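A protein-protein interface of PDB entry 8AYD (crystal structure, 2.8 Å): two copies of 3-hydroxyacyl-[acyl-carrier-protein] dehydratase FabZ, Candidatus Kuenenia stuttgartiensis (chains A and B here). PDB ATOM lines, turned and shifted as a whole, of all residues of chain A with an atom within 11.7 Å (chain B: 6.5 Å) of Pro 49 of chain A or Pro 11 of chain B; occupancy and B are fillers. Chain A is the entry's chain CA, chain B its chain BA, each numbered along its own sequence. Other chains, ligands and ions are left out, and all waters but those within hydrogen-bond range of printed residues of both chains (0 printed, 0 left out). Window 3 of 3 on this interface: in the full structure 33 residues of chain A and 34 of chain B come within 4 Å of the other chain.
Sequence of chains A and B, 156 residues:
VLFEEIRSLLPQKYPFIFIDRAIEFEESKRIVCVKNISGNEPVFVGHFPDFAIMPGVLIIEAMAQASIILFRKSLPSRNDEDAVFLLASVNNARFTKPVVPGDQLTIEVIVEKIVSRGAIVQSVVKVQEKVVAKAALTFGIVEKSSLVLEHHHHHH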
ATOM      1  N   GLY A  39      40.827 -25.770 -12.603  1.00  0.00           N
ATOM      2  CA  GLY A  39      39.988 -24.700 -12.093  1.00  0.00           C
ATOM      3  C   GLY A  39      40.530 -23.305 -12.315  1.00  0.00           C
ATOM      4  O   GLY A  39      39.754 -22.348 -12.385  1.00  0.00           O
ATOM      5  N   GLU A  41      41.611 -22.073 -14.972  1.00  0.00           N
ATOM      6  CA  GLU A  41      41.631 -21.480 -16.298  1.00  0.00           C
ATOM      7  C   GLU A  41      40.670 -20.296 -16.353  1.00  0.00           C
ATOM      8  O   GLU A  41      39.679 -20.261 -15.617  1.00  0.00           O
ATOM      9  CB  GLU A  41      41.245 -22.512 -17.349  1.00  0.00           C
ATOM     10  CG  GLU A  41      42.202 -23.678 -17.400  1.00  0.00           C
ATOM     11  CD  GLU A  41      41.869 -24.655 -18.498  1.00  0.00           C
ATOM     12  OE1 GLU A  41      40.888 -24.419 -19.235  1.00  0.00           O
ATOM     13  OE2 GLU A  41      42.576 -25.676 -18.599  1.00  0.00           O
ATOM     14  N   PRO A  42      40.942 -19.303 -17.210  1.00  0.00           N
ATOM     15  CA  PRO A  42      40.143 -18.065 -17.169  1.00  0.00           C
ATOM     16  C   PRO A  42      38.684 -18.246 -17.534  1.00  0.00           C
ATOM     17  O   PRO A  42      37.855 -17.454 -17.075  1.00  0.00           O
ATOM     18  CB  PRO A  42      40.867 -17.144 -18.162  1.00  0.00           C
ATOM     19  CG  PRO A  42      41.614 -18.062 -19.060  1.00  0.00           C
ATOM     20  CD  PRO A  42      42.019 -19.231 -18.211  1.00  0.00           C
ATOM     21  N   VAL A  43      38.336 -19.277 -18.303  1.00  0.00           N
ATOM     22  CA  VAL A  43      36.970 -19.384 -18.801  1.00  0.00           C
ATOM     23  C   VAL A  43      35.994 -19.750 -17.686  1.00  0.00           C
ATOM     24  O   VAL A  43      34.823 -19.352 -17.723  1.00  0.00           O
ATOM     25  CB  VAL A  43      36.917 -20.393 -19.964  1.00  0.00           C
ATOM     26  CG1 VAL A  43      37.295 -21.790 -19.487  1.00  0.00           C
ATOM     27  CG2 VAL A  43      35.543 -20.387 -20.606  1.00  0.00           C
ATOM     28  N   PHE A  44      36.449 -20.486 -16.673  1.00  0.00           N
ATOM     29  CA  PHE A  44      35.563 -20.989 -15.628  1.00  0.00           C
ATOM     30  C   PHE A  44      35.168 -19.929 -14.609  1.00  0.00           C
ATOM     31  O   PHE A  44      34.370 -20.225 -13.713  1.00  0.00           O
ATOM     32  CB  PHE A  44      36.223 -22.172 -14.923  1.00  0.00           C
ATOM     33  CG  PHE A  44      36.336 -23.388 -15.786  1.00  0.00           C
ATOM     34  CD1 PHE A  44      35.516 -23.541 -16.892  1.00  0.00           C
ATOM     35  CD2 PHE A  44      37.283 -24.358 -15.519  1.00  0.00           C
ATOM     36  CE1 PHE A  44      35.620 -24.652 -17.699  1.00  0.00           C
ATOM     37  CE2 PHE A  44      37.393 -25.467 -16.327  1.00  0.00           C
ATOM     38  CZ  PHE A  44      36.560 -25.618 -17.416  1.00  0.00           C
ATOM     39  N   VAL A  45      35.699 -18.711 -14.721  1.00  0.00           N
ATOM     40  CA  VAL A  45      35.289 -17.648 -13.812  1.00  0.00           C
ATOM     41  C   VAL A  45      33.877 -17.186 -14.143  1.00  0.00           C
ATOM     42  O   VAL A  45      33.124 -16.770 -13.253  1.00  0.00           O
ATOM     43  CB  VAL A  45      36.301 -16.488 -13.867  1.00  0.00           C
ATOM     44  CG1 VAL A  45      35.902 -15.371 -12.909  1.00  0.00           C
ATOM     45  CG2 VAL A  45      37.704 -16.992 -13.570  1.00  0.00           C
ATOM     46  N   GLY A  46      33.485 -17.266 -15.413  1.00  0.00           N
ATOM     47  CA  GLY A  46      32.168 -16.829 -15.826  1.00  0.00           C
ATOM     48  C   GLY A  46      31.366 -17.878 -16.570  1.00  0.00           C
ATOM     49  O   GLY A  46      30.247 -17.604 -17.013  1.00  0.00           O
ATOM     50  N   HIS A  47      31.923 -19.082 -16.726  1.00  0.00           N
ATOM     51  CA  HIS A  47      31.214 -20.185 -17.384  1.00  0.00           C
ATOM     52  C   HIS A  47      31.474 -21.470 -16.598  1.00  0.00           C
ATOM     53  O   HIS A  47      32.402 -22.220 -16.912  1.00  0.00           O
ATOM     54  CB  HIS A  47      31.654 -20.321 -18.837  1.00  0.00           C
ATOM     55  CG  HIS A  47      30.858 -21.315 -19.623  1.00  0.00           C
ATOM     56  ND1 HIS A  47      31.126 -22.667 -19.603  1.00  0.00           N
ATOM     57  CD2 HIS A  47      29.812 -21.151 -20.468  1.00  0.00           C
ATOM     58  CE1 HIS A  47      30.273 -23.295 -20.392  1.00  0.00           C
ATOM     59  NE2 HIS A  47      29.466 -22.398 -20.930  1.00  0.00           N
ATOM     60  N   PHE A  48      30.651 -21.726 -15.584  1.00  0.00           N
ATOM     61  CA  PHE A  48      29.687 -20.758 -15.070  1.00  0.00           C
ATOM     62  C   PHE A  48      30.071 -20.421 -13.633  1.00  0.00           C
ATOM     63  O   PHE A  48      30.775 -21.195 -12.985  1.00  0.00           O
ATOM     64  CB  PHE A  48      28.260 -21.311 -15.116  1.00  0.00           C
ATOM     65  CG  PHE A  48      27.764 -21.609 -16.501  1.00  0.00           C
ATOM     66  CD1 PHE A  48      27.316 -20.594 -17.328  1.00  0.00           C
ATOM     67  CD2 PHE A  48      27.729 -22.913 -16.968  1.00  0.00           C
ATOM     68  CE1 PHE A  48      26.854 -20.873 -18.600  1.00  0.00           C
ATOM     69  CE2 PHE A  48      27.268 -23.199 -18.236  1.00  0.00           C
ATOM     70  CZ  PHE A  48      26.829 -22.177 -19.055  1.00  0.00           C
ATOM     71  N   PRO A  49      29.625 -19.267 -13.132  1.00  0.00           N
ATOM     72  CA  PRO A  49      29.805 -18.993 -11.697  1.00  0.00           C
ATOM     73  C   PRO A  49      29.064 -19.978 -10.811  1.00  0.00           C
ATOM     74  O   PRO A  49      29.532 -20.279  -9.707  1.00  0.00           O
ATOM     75  CB  PRO A  49      29.264 -17.565 -11.541  1.00  0.00           C
ATOM     76  CG  PRO A  49      29.387 -16.966 -12.902  1.00  0.00           C
ATOM     77  CD  PRO A  49      29.112 -18.092 -13.855  1.00  0.00           C
ATOM     78  N   ASP A  50      27.914 -20.489 -11.263  1.00  0.00           N
ATOM     79  CA  ASP A  50      27.204 -21.508 -10.498  1.00  0.00           C
ATOM     80  C   ASP A  50      28.019 -22.792 -10.410  1.00  0.00           C
ATOM     81  O   ASP A  50      28.147 -23.386  -9.333  1.00  0.00           O
ATOM     82  CB  ASP A  50      25.831 -21.771 -11.120  1.00  0.00           C
ATOM     83  CG  ASP A  50      24.850 -20.640 -10.869  1.00  0.00           C
ATOM     84  OD1 ASP A  50      24.957 -19.986  -9.809  1.00  0.00           O
ATOM     85  OD2 ASP A  50      23.978 -20.402 -11.729  1.00  0.00           O
ATOM     86  N   PHE A  51      28.583 -23.234 -11.532  1.00  0.00           N
ATOM     87  CA  PHE A  51      29.468 -24.392 -11.549  1.00  0.00           C
ATOM     88  C   PHE A  51      30.176 -24.430 -12.896  1.00  0.00           C
ATOM     89  O   PHE A  51      29.651 -23.935 -13.897  1.00  0.00           O
ATOM     90  CB  PHE A  51      28.695 -25.693 -11.292  1.00  0.00           C
ATOM     91  CG  PHE A  51      27.867 -26.155 -12.452  1.00  0.00           C
ATOM     92  CD1 PHE A  51      26.661 -25.546 -12.756  1.00  0.00           C
ATOM     93  CD2 PHE A  51      28.266 -27.249 -13.195  1.00  0.00           C
ATOM     94  CE1 PHE A  51      25.898 -25.989 -13.820  1.00  0.00           C
ATOM     95  CE2 PHE A  51      27.505 -27.701 -14.241  1.00  0.00           C
ATOM     96  CZ  PHE A  51      26.320 -27.071 -14.562  1.00  0.00           C
ATOM     97  N   ALA A  52      31.369 -25.021 -12.909  1.00  0.00           N
ATOM     98  CA  ALA A  52      32.281 -24.903 -14.041  1.00  0.00           C
ATOM     99  C   ALA A  52      32.074 -26.046 -15.032  1.00  0.00           C
ATOM    100  O   ALA A  52      32.240 -27.219 -14.679  1.00  0.00           O
ATOM    101  CB  ALA A  52      33.730 -24.879 -13.554  1.00  0.00           C
ATOM    102  N   ILE A  53      31.720 -25.698 -16.269  1.00  0.00           N
ATOM    103  CA  ILE A  53      31.719 -26.626 -17.395  1.00  0.00           C
ATOM    104  C   ILE A  53      32.565 -26.047 -18.518  1.00  0.00           C
ATOM    105  O   ILE A  53      32.468 -24.855 -18.834  1.00  0.00           O
ATOM    106  CB  ILE A  53      30.295 -26.943 -17.908  1.00  0.00           C
ATOM    107  CG1 ILE A  53      29.586 -27.926 -16.983  1.00  0.00           C
ATOM    108  CG2 ILE A  53      30.320 -27.472 -19.337  1.00  0.00           C
ATOM    109  CD1 ILE A  53      28.178 -28.231 -17.428  1.00  0.00           C
ATOM    110  N   MET A  54      33.396 -26.892 -19.113  1.00  0.00           N
ATOM    111  CA  MET A  54      34.152 -26.535 -20.303  1.00  0.00           C
ATOM    112  C   MET A  54      33.191 -26.236 -21.448  1.00  0.00           C
ATOM    113  O   MET A  54      32.396 -27.113 -21.821  1.00  0.00           O
ATOM    114  CB  MET A  54      35.089 -27.680 -20.677  1.00  0.00           C
ATOM    115  CG  MET A  54      36.134 -27.352 -21.729  1.00  0.00           C
ATOM    116  SD  MET A  54      37.374 -26.199 -21.114  1.00  0.00           S
ATOM    117  CE  MET A  54      38.067 -25.593 -22.647  1.00  0.00           C
ATOM    118  N   PRO A  55      33.209 -25.031 -22.017  1.00  0.00           N
ATOM    119  CA  PRO A  55      32.290 -24.725 -23.120  1.00  0.00           C
ATOM    120  C   PRO A  55      32.529 -25.639 -24.313  1.00  0.00           C
ATOM    121  O   PRO A  55      33.666 -25.998 -24.629  1.00  0.00           O
ATOM    122  CB  PRO A  55      32.614 -23.264 -23.456  1.00  0.00           C
ATOM    123  CG  PRO A  55      33.211 -22.715 -22.202  1.00  0.00           C
ATOM    124  CD  PRO A  55      33.987 -23.851 -21.604  1.00  0.00           C
ATOM    125  N   PRO A 101      36.344 -29.498 -14.528  1.00  0.00           N
ATOM    126  CA  PRO A 101      37.700 -29.515 -13.962  1.00  0.00           C
ATOM    127  C   PRO A 101      37.998 -30.826 -13.246  1.00  0.00           C
ATOM    128  O   PRO A 101      37.141 -31.402 -12.572  1.00  0.00           O
ATOM    129  CB  PRO A 101      37.689 -28.329 -12.994  1.00  0.00           C
ATOM    130  CG  PRO A 101      36.730 -27.384 -13.606  1.00  0.00           C
ATOM    131  CD  PRO A 101      35.659 -28.220 -14.254  1.00  0.00           C
ATOM    132  N   ILE B   6      20.737  -8.236 -20.685  1.00  0.00           N
ATOM    133  CA  ILE B   6      21.559  -9.285 -21.287  1.00  0.00           C
ATOM    134  C   ILE B   6      22.372 -10.009 -20.223  1.00  0.00           C
ATOM    135  O   ILE B   6      22.499 -11.239 -20.245  1.00  0.00           O
ATOM    136  CB  ILE B   6      22.470  -8.686 -22.377  1.00  0.00           C
ATOM    137  CG1 ILE B   6      21.642  -8.041 -23.488  1.00  0.00           C
ATOM    138  CG2 ILE B   6      23.385  -9.752 -22.953  1.00  0.00           C
ATOM    139  CD1 ILE B   6      20.780  -9.020 -24.247  1.00  0.00           C
ATOM    140  N   ARG B   7      22.928  -9.259 -19.269  1.00  0.00           N
ATOM    141  CA  ARG B   7      23.803  -9.860 -18.271  1.00  0.00           C
ATOM    142  C   ARG B   7      23.022 -10.619 -17.205  1.00  0.00           C
ATOM    143  O   ARG B   7      23.522 -11.615 -16.671  1.00  0.00           O
ATOM    144  CB  ARG B   7      24.691  -8.778 -17.645  1.00  0.00           C
ATOM    145  CG  ARG B   7      25.784  -9.313 -16.738  1.00  0.00           C
ATOM    146  CD  ARG B   7      26.759  -8.218 -16.325  1.00  0.00           C
ATOM    147  NE  ARG B   7      26.160  -7.208 -15.461  1.00  0.00           N
ATOM    148  CZ  ARG B   7      26.764  -6.073 -15.116  1.00  0.00           C
ATOM    149  NH1 ARG B   7      27.984  -5.804 -15.568  1.00  0.00           N
ATOM    150  NH2 ARG B   7      26.152  -5.205 -14.319  1.00  0.00           N
ATOM    151  N   SER B   8      21.806 -10.174 -16.884  1.00  0.00           N
ATOM    152  CA  SER B   8      20.963 -10.930 -15.964  1.00  0.00           C
ATOM    153  C   SER B   8      20.314 -12.131 -16.644  1.00  0.00           C
ATOM    154  O   SER B   8      20.023 -13.134 -15.980  1.00  0.00           O
ATOM    155  CB  SER B   8      19.886 -10.024 -15.361  1.00  0.00           C
ATOM    156  OG  SER B   8      18.970  -9.588 -16.351  1.00  0.00           O
ATOM    157  N   LEU B   9      20.078 -12.052 -17.956  1.00  0.00           N
ATOM    158  CA  LEU B   9      19.459 -13.161 -18.676  1.00  0.00           C
ATOM    159  C   LEU B   9      20.474 -14.240 -19.037  1.00  0.00           C
ATOM    160  O   LEU B   9      20.153 -15.432 -18.988  1.00  0.00           O
ATOM    161  CB  LEU B   9      18.765 -12.644 -19.936  1.00  0.00           C
ATOM    162  CG  LEU B   9      17.511 -11.786 -19.765  1.00  0.00           C
ATOM    163  CD1 LEU B   9      17.126 -11.156 -21.091  1.00  0.00           C
ATOM    164  CD2 LEU B   9      16.367 -12.623 -19.219  1.00  0.00           C
ATOM    165  N   LEU B  10      21.698 -13.846 -19.406  1.00  0.00           N
ATOM    166  CA  LEU B  10      22.695 -14.845 -19.770  1.00  0.00           C
ATOM    167  C   LEU B  10      23.264 -15.519 -18.524  1.00  0.00           C
ATOM    168  O   LEU B  10      23.544 -14.850 -17.527  1.00  0.00           O
ATOM    169  CB  LEU B  10      23.836 -14.220 -20.570  1.00  0.00           C
ATOM    170  CG  LEU B  10      23.568 -13.815 -22.015  1.00  0.00           C
ATOM    171  CD1 LEU B  10      24.775 -13.102 -22.599  1.00  0.00           C
ATOM    172  CD2 LEU B  10      23.220 -15.042 -22.841  1.00  0.00           C
ATOM    173  N   PRO B  11      23.443 -16.843 -18.560  1.00  0.00           N
ATOM    174  CA  PRO B  11      24.197 -17.508 -17.490  1.00  0.00           C
ATOM    175  C   PRO B  11      25.698 -17.310 -17.604  1.00  0.00           C
ATOM    176  O   PRO B  11      26.410 -17.551 -16.621  1.00  0.00           O
ATOM    177  CB  PRO B  11      23.822 -18.986 -17.661  1.00  0.00           C
ATOM    178  CG  PRO B  11      23.507 -19.111 -19.118  1.00  0.00           C
ATOM    179  CD  PRO B  11      22.877 -17.804 -19.523  1.00  0.00           C
ATOM    180  N   GLN B  12      26.195 -16.882 -18.764  1.00  0.00           N
ATOM    181  CA  GLN B  12      27.619 -16.652 -18.961  1.00  0.00           C
ATOM    182  C   GLN B  12      27.979 -15.237 -18.528  1.00  0.00           C
ATOM    183  O   GLN B  12      27.341 -14.269 -18.951  1.00  0.00           O
ATOM    184  CB  GLN B  12      28.013 -16.861 -20.425  1.00  0.00           C
ATOM    185  CG  GLN B  12      27.849 -18.281 -20.940  1.00  0.00           C
ATOM    186  CD  GLN B  12      26.449 -18.557 -21.450  1.00  0.00           C
ATOM    187  OE1 GLN B  12      25.680 -17.633 -21.714  1.00  0.00           O
ATOM    188  NE2 GLN B  12      26.113 -19.833 -21.598  1.00  0.00           N
ATOM    189  N   LYS B  13      28.998 -15.126 -17.684  1.00  0.00           N
ATOM    190  CA  LYS B  13      29.550 -13.848 -17.262  1.00  0.00           C
ATOM    191  C   LYS B  13      30.994 -13.777 -17.750  1.00  0.00           C
ATOM    192  O   LYS B  13      31.526 -14.749 -18.291  1.00  0.00           O
ATOM    193  CB  LYS B  13      29.454 -13.683 -15.737  1.00  0.00           C
ATOM    194  CG  LYS B  13      28.045 -13.339 -15.229  1.00  0.00           C
ATOM    195  CD  LYS B  13      27.113 -14.551 -15.267  1.00  0.00           C
ATOM    196  CE  LYS B  13      25.730 -14.234 -14.720  1.00  0.00           C
ATOM    197  NZ  LYS B  13      24.792 -15.380 -14.897  1.00  0.00           N
ATOM    198  N   TYR B  14      31.634 -12.620 -17.584  1.00  0.00           N
ATOM    199  CA  TYR B  14      32.980 -12.478 -18.127  1.00  0.00           C
ATOM    200  C   TYR B  14      33.952 -13.419 -17.414  1.00  0.00           C
ATOM    201  O   TYR B  14      33.844 -13.631 -16.202  1.00  0.00           O
ATOM    202  CB  TYR B  14      33.410 -10.980 -18.156  1.00  0.00           C
ATOM    203  CG  TYR B  14      34.877 -10.510 -18.008  1.00  0.00           C
ATOM    204  CD1 TYR B  14      35.931 -11.355 -17.697  1.00  0.00           C
ATOM    205  CD2 TYR B  14      35.229  -9.280 -18.527  1.00  0.00           C
ATOM    206  CE1 TYR B  14      37.229 -10.942 -17.664  1.00  0.00           C
ATOM    207  CE2 TYR B  14      36.536  -8.861 -18.528  1.00  0.00           C
ATOM    208  CZ  TYR B  14      37.537  -9.696 -18.091  1.00  0.00           C
ATOM    209  OH  TYR B  14      38.852  -9.288 -18.082  1.00  0.00           O
ATOM    210  N   ILE B  68      19.891 -18.094 -26.258  1.00  0.00           N
ATOM    211  CA  ILE B  68      19.585 -18.237 -24.837  1.00  0.00           C
ATOM    212  C   ILE B  68      18.805 -17.025 -24.344  1.00  0.00           C
ATOM    213  O   ILE B  68      17.888 -17.148 -23.524  1.00  0.00           O
ATOM    214  CB  ILE B  68      20.877 -18.463 -24.027  1.00  0.00           C
ATOM    215  CG1 ILE B  68      21.498 -19.815 -24.384  1.00  0.00           C
ATOM    216  CG2 ILE B  68      20.605 -18.382 -22.533  1.00  0.00           C
ATOM    217  CD1 ILE B  68      22.882 -20.027 -23.809  1.00  0.00           C
ATOM    218  N   ARG B  72      14.909 -17.604 -23.199  1.00  0.00           N
ATOM    219  CA  ARG B  72      14.625 -17.313 -21.800  1.00  0.00           C
ATOM    220  C   ARG B  72      13.769 -16.071 -21.589  1.00  0.00           C
ATOM    221  O   ARG B  72      13.166 -15.934 -20.519  1.00  0.00           O
ATOM    222  CB  ARG B  72      15.937 -17.169 -21.019  1.00  0.00           C
ATOM    223  CG  ARG B  72      15.750 -17.168 -19.522  1.00  0.00           C
ATOM    224  CD  ARG B  72      17.060 -17.047 -18.784  1.00  0.00           C
ATOM    225  NE  ARG B  72      16.834 -17.046 -17.346  1.00  0.00           N
ATOM    226  CZ  ARG B  72      17.783 -16.853 -16.439  1.00  0.00           C
ATOM    227  NH1 ARG B  72      19.032 -16.621 -16.819  1.00  0.00           N
ATOM    228  NH2 ARG B  72      17.478 -16.873 -15.147  1.00  0.00           N
ATOM    229  N   ALA B  83      19.092 -22.823 -14.698  1.00  0.00           N
ATOM    230  CA  ALA B  83      19.147 -23.431 -16.022  1.00  0.00           C
ATOM    231  C   ALA B  83      20.399 -22.989 -16.769  1.00  0.00           C
ATOM    232  O   ALA B  83      20.655 -21.794 -16.918  1.00  0.00           O
ATOM    233  CB  ALA B  83      17.900 -23.080 -16.819  1.00  0.00           C
ATOM    234  N   VAL B  84      21.180 -23.959 -17.233  1.00  0.00           N
ATOM    235  CA  VAL B  84      22.400 -23.703 -17.991  1.00  0.00           C
ATOM    236  C   VAL B  84      22.216 -24.335 -19.366  1.00  0.00           C
ATOM    237  O   VAL B  84      22.392 -25.545 -19.538  1.00  0.00           O
ATOM    238  CB  VAL B  84      23.653 -24.232 -17.274  1.00  0.00           C
ATOM    239  CG1 VAL B  84      23.944 -23.390 -16.048  1.00  0.00           C
ATOM    240  CG2 VAL B  84      23.475 -25.685 -16.831  1.00  0.00           C
ATOM    241  N   PHE B  85      21.847 -23.535 -20.362  1.00  0.00           N
ATOM    242  CA  PHE B  85      21.616 -24.105 -21.684  1.00  0.00           C
ATOM    243  C   PHE B  85      22.964 -24.429 -22.313  1.00  0.00           C
ATOM    244  O   PHE B  85      23.788 -23.534 -22.532  1.00  0.00           O
ATOM    245  CB  PHE B  85      20.807 -23.184 -22.598  1.00  0.00           C
ATOM    246  CG  PHE B  85      19.386 -22.961 -22.151  1.00  0.00           C
ATOM    247  CD1 PHE B  85      18.957 -23.342 -20.889  1.00  0.00           C
ATOM    248  CD2 PHE B  85      18.445 -22.488 -23.048  1.00  0.00           C
ATOM    249  CE1 PHE B  85      17.648 -23.150 -20.498  1.00  0.00           C
ATOM    250  CE2 PHE B  85      17.129 -22.316 -22.669  1.00  0.00           C
ATOM    251  CZ  PHE B  85      16.729 -22.646 -21.393  1.00  0.00           C
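Printed residues of chain A within 4 Å of Pro 11 of chain B: Gly 46 (3.9 Å), Phe 48 (3.3 Å) and Pro 49 (3.9 Å).
No residue of chain A comes within 4 Å of Leu 10 of chain B.
Gln 12 of chain B touches just these residues of chain A: Gly 46, His 47 and Phe 48.
Lys 13 of chain B touches one residue of chain A.
No residue of chain A comes within 4 Å of Ile 68 of chain B.
No residue of chain A comes within 4 Å of Ala 83 of chain B.
Printed residues of chain A within 4 Å of Val 84 of chain B: Phe 48 (3.9 Å) and Phe 51 (3.9 Å).
Printed residues of chain B within 4 Å of Phe 51 of chain A: Val 84 (3.9 Å).
Printed residues of chain B within 4 Å of Gly 46 of chain A: Pro 11 (3.9 Å), Gln 12 (3.4 Å), Lys 13 (2.9 Å) and Tyr 14 (3.6 Å).
Printed residues of chain B within 4 Å of Phe 48 of chain A: Pro 11 (3.3 Å), Gln 12 (3.3 Å) and Val 84 (3.9 Å).
Of the printed residues of chain B, His 47 of chain A touches Gln 12.
Ala 52 of chain A touches none of the printed residues of chain B.
Val 45 of chain A touches none of the printed residues of chain B.
The nearest residue of chain B that does not touch Pro 49 of chain A is Lys 13 of chain B (4.1 Å).
The nearest residue of chain A that does not touch Pro 11 of chain B is His 47 of chain A (5.5 Å).
The backbone carbonyl oxygen of Pro 11 of chain B lies within hydrogen-bond range of the side-chain amino group of Lys 13 of chain B, at 3.2 Å.
NZ of Lys 13 of chain B is in hydrogen-bond range of O of Leu 10 of chain B (3.0 Å).
ND1 of His 47 of chain A is in hydrogen-bond range of O of Ile 53 of chain A, 2.7 Å away.
Among the printed residues, merely in contact across the chains: Gly 46 of chain A with Pro 11 of chain B (3.9 Å), Gly 46 of chain A with Gln 12 of chain B (3.4 Å), Gly 46 of chain A with Tyr 14 of chain B (3.6 Å), His 47 of chain A with Gln 12 of chain B (3.5 Å), Phe 48 of chain A with Pro 11 of chain B (3.3 Å), Phe 48 of chain A with Gln 12 of chain B (3.3 Å), Phe 48 of chain A with Val 84 of chain B (3.9 Å), Pro 49 of chain A with Pro 11 of chain B (3.9 Å) and Phe 51 of chain A with Val 84 of chain B (3.9 Å).
Hydrophobic or aromatic side chains of chain B that line the printed part of chain A: Pro 11 and Val 84.
Of the 17 printed residues of chain A, 5 touch a printed residue of chain B.
Along chain A the printed residues that touch a printed residue of chain B span positions 46 to 51.
Among the printed residues, 10 pairs touch across the chains.
Among the printed residues, no Asp or Glu carboxylate lies within 4 Å of a Lys or Arg side-chain nitrogen of the other chain.
No position is printed for both chains.
The backbone NH (N) of Lys 13 of chain B lies within hydrogen-bond range of the backbone carbonyl oxygen (O) of Gly 46 of chain A.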
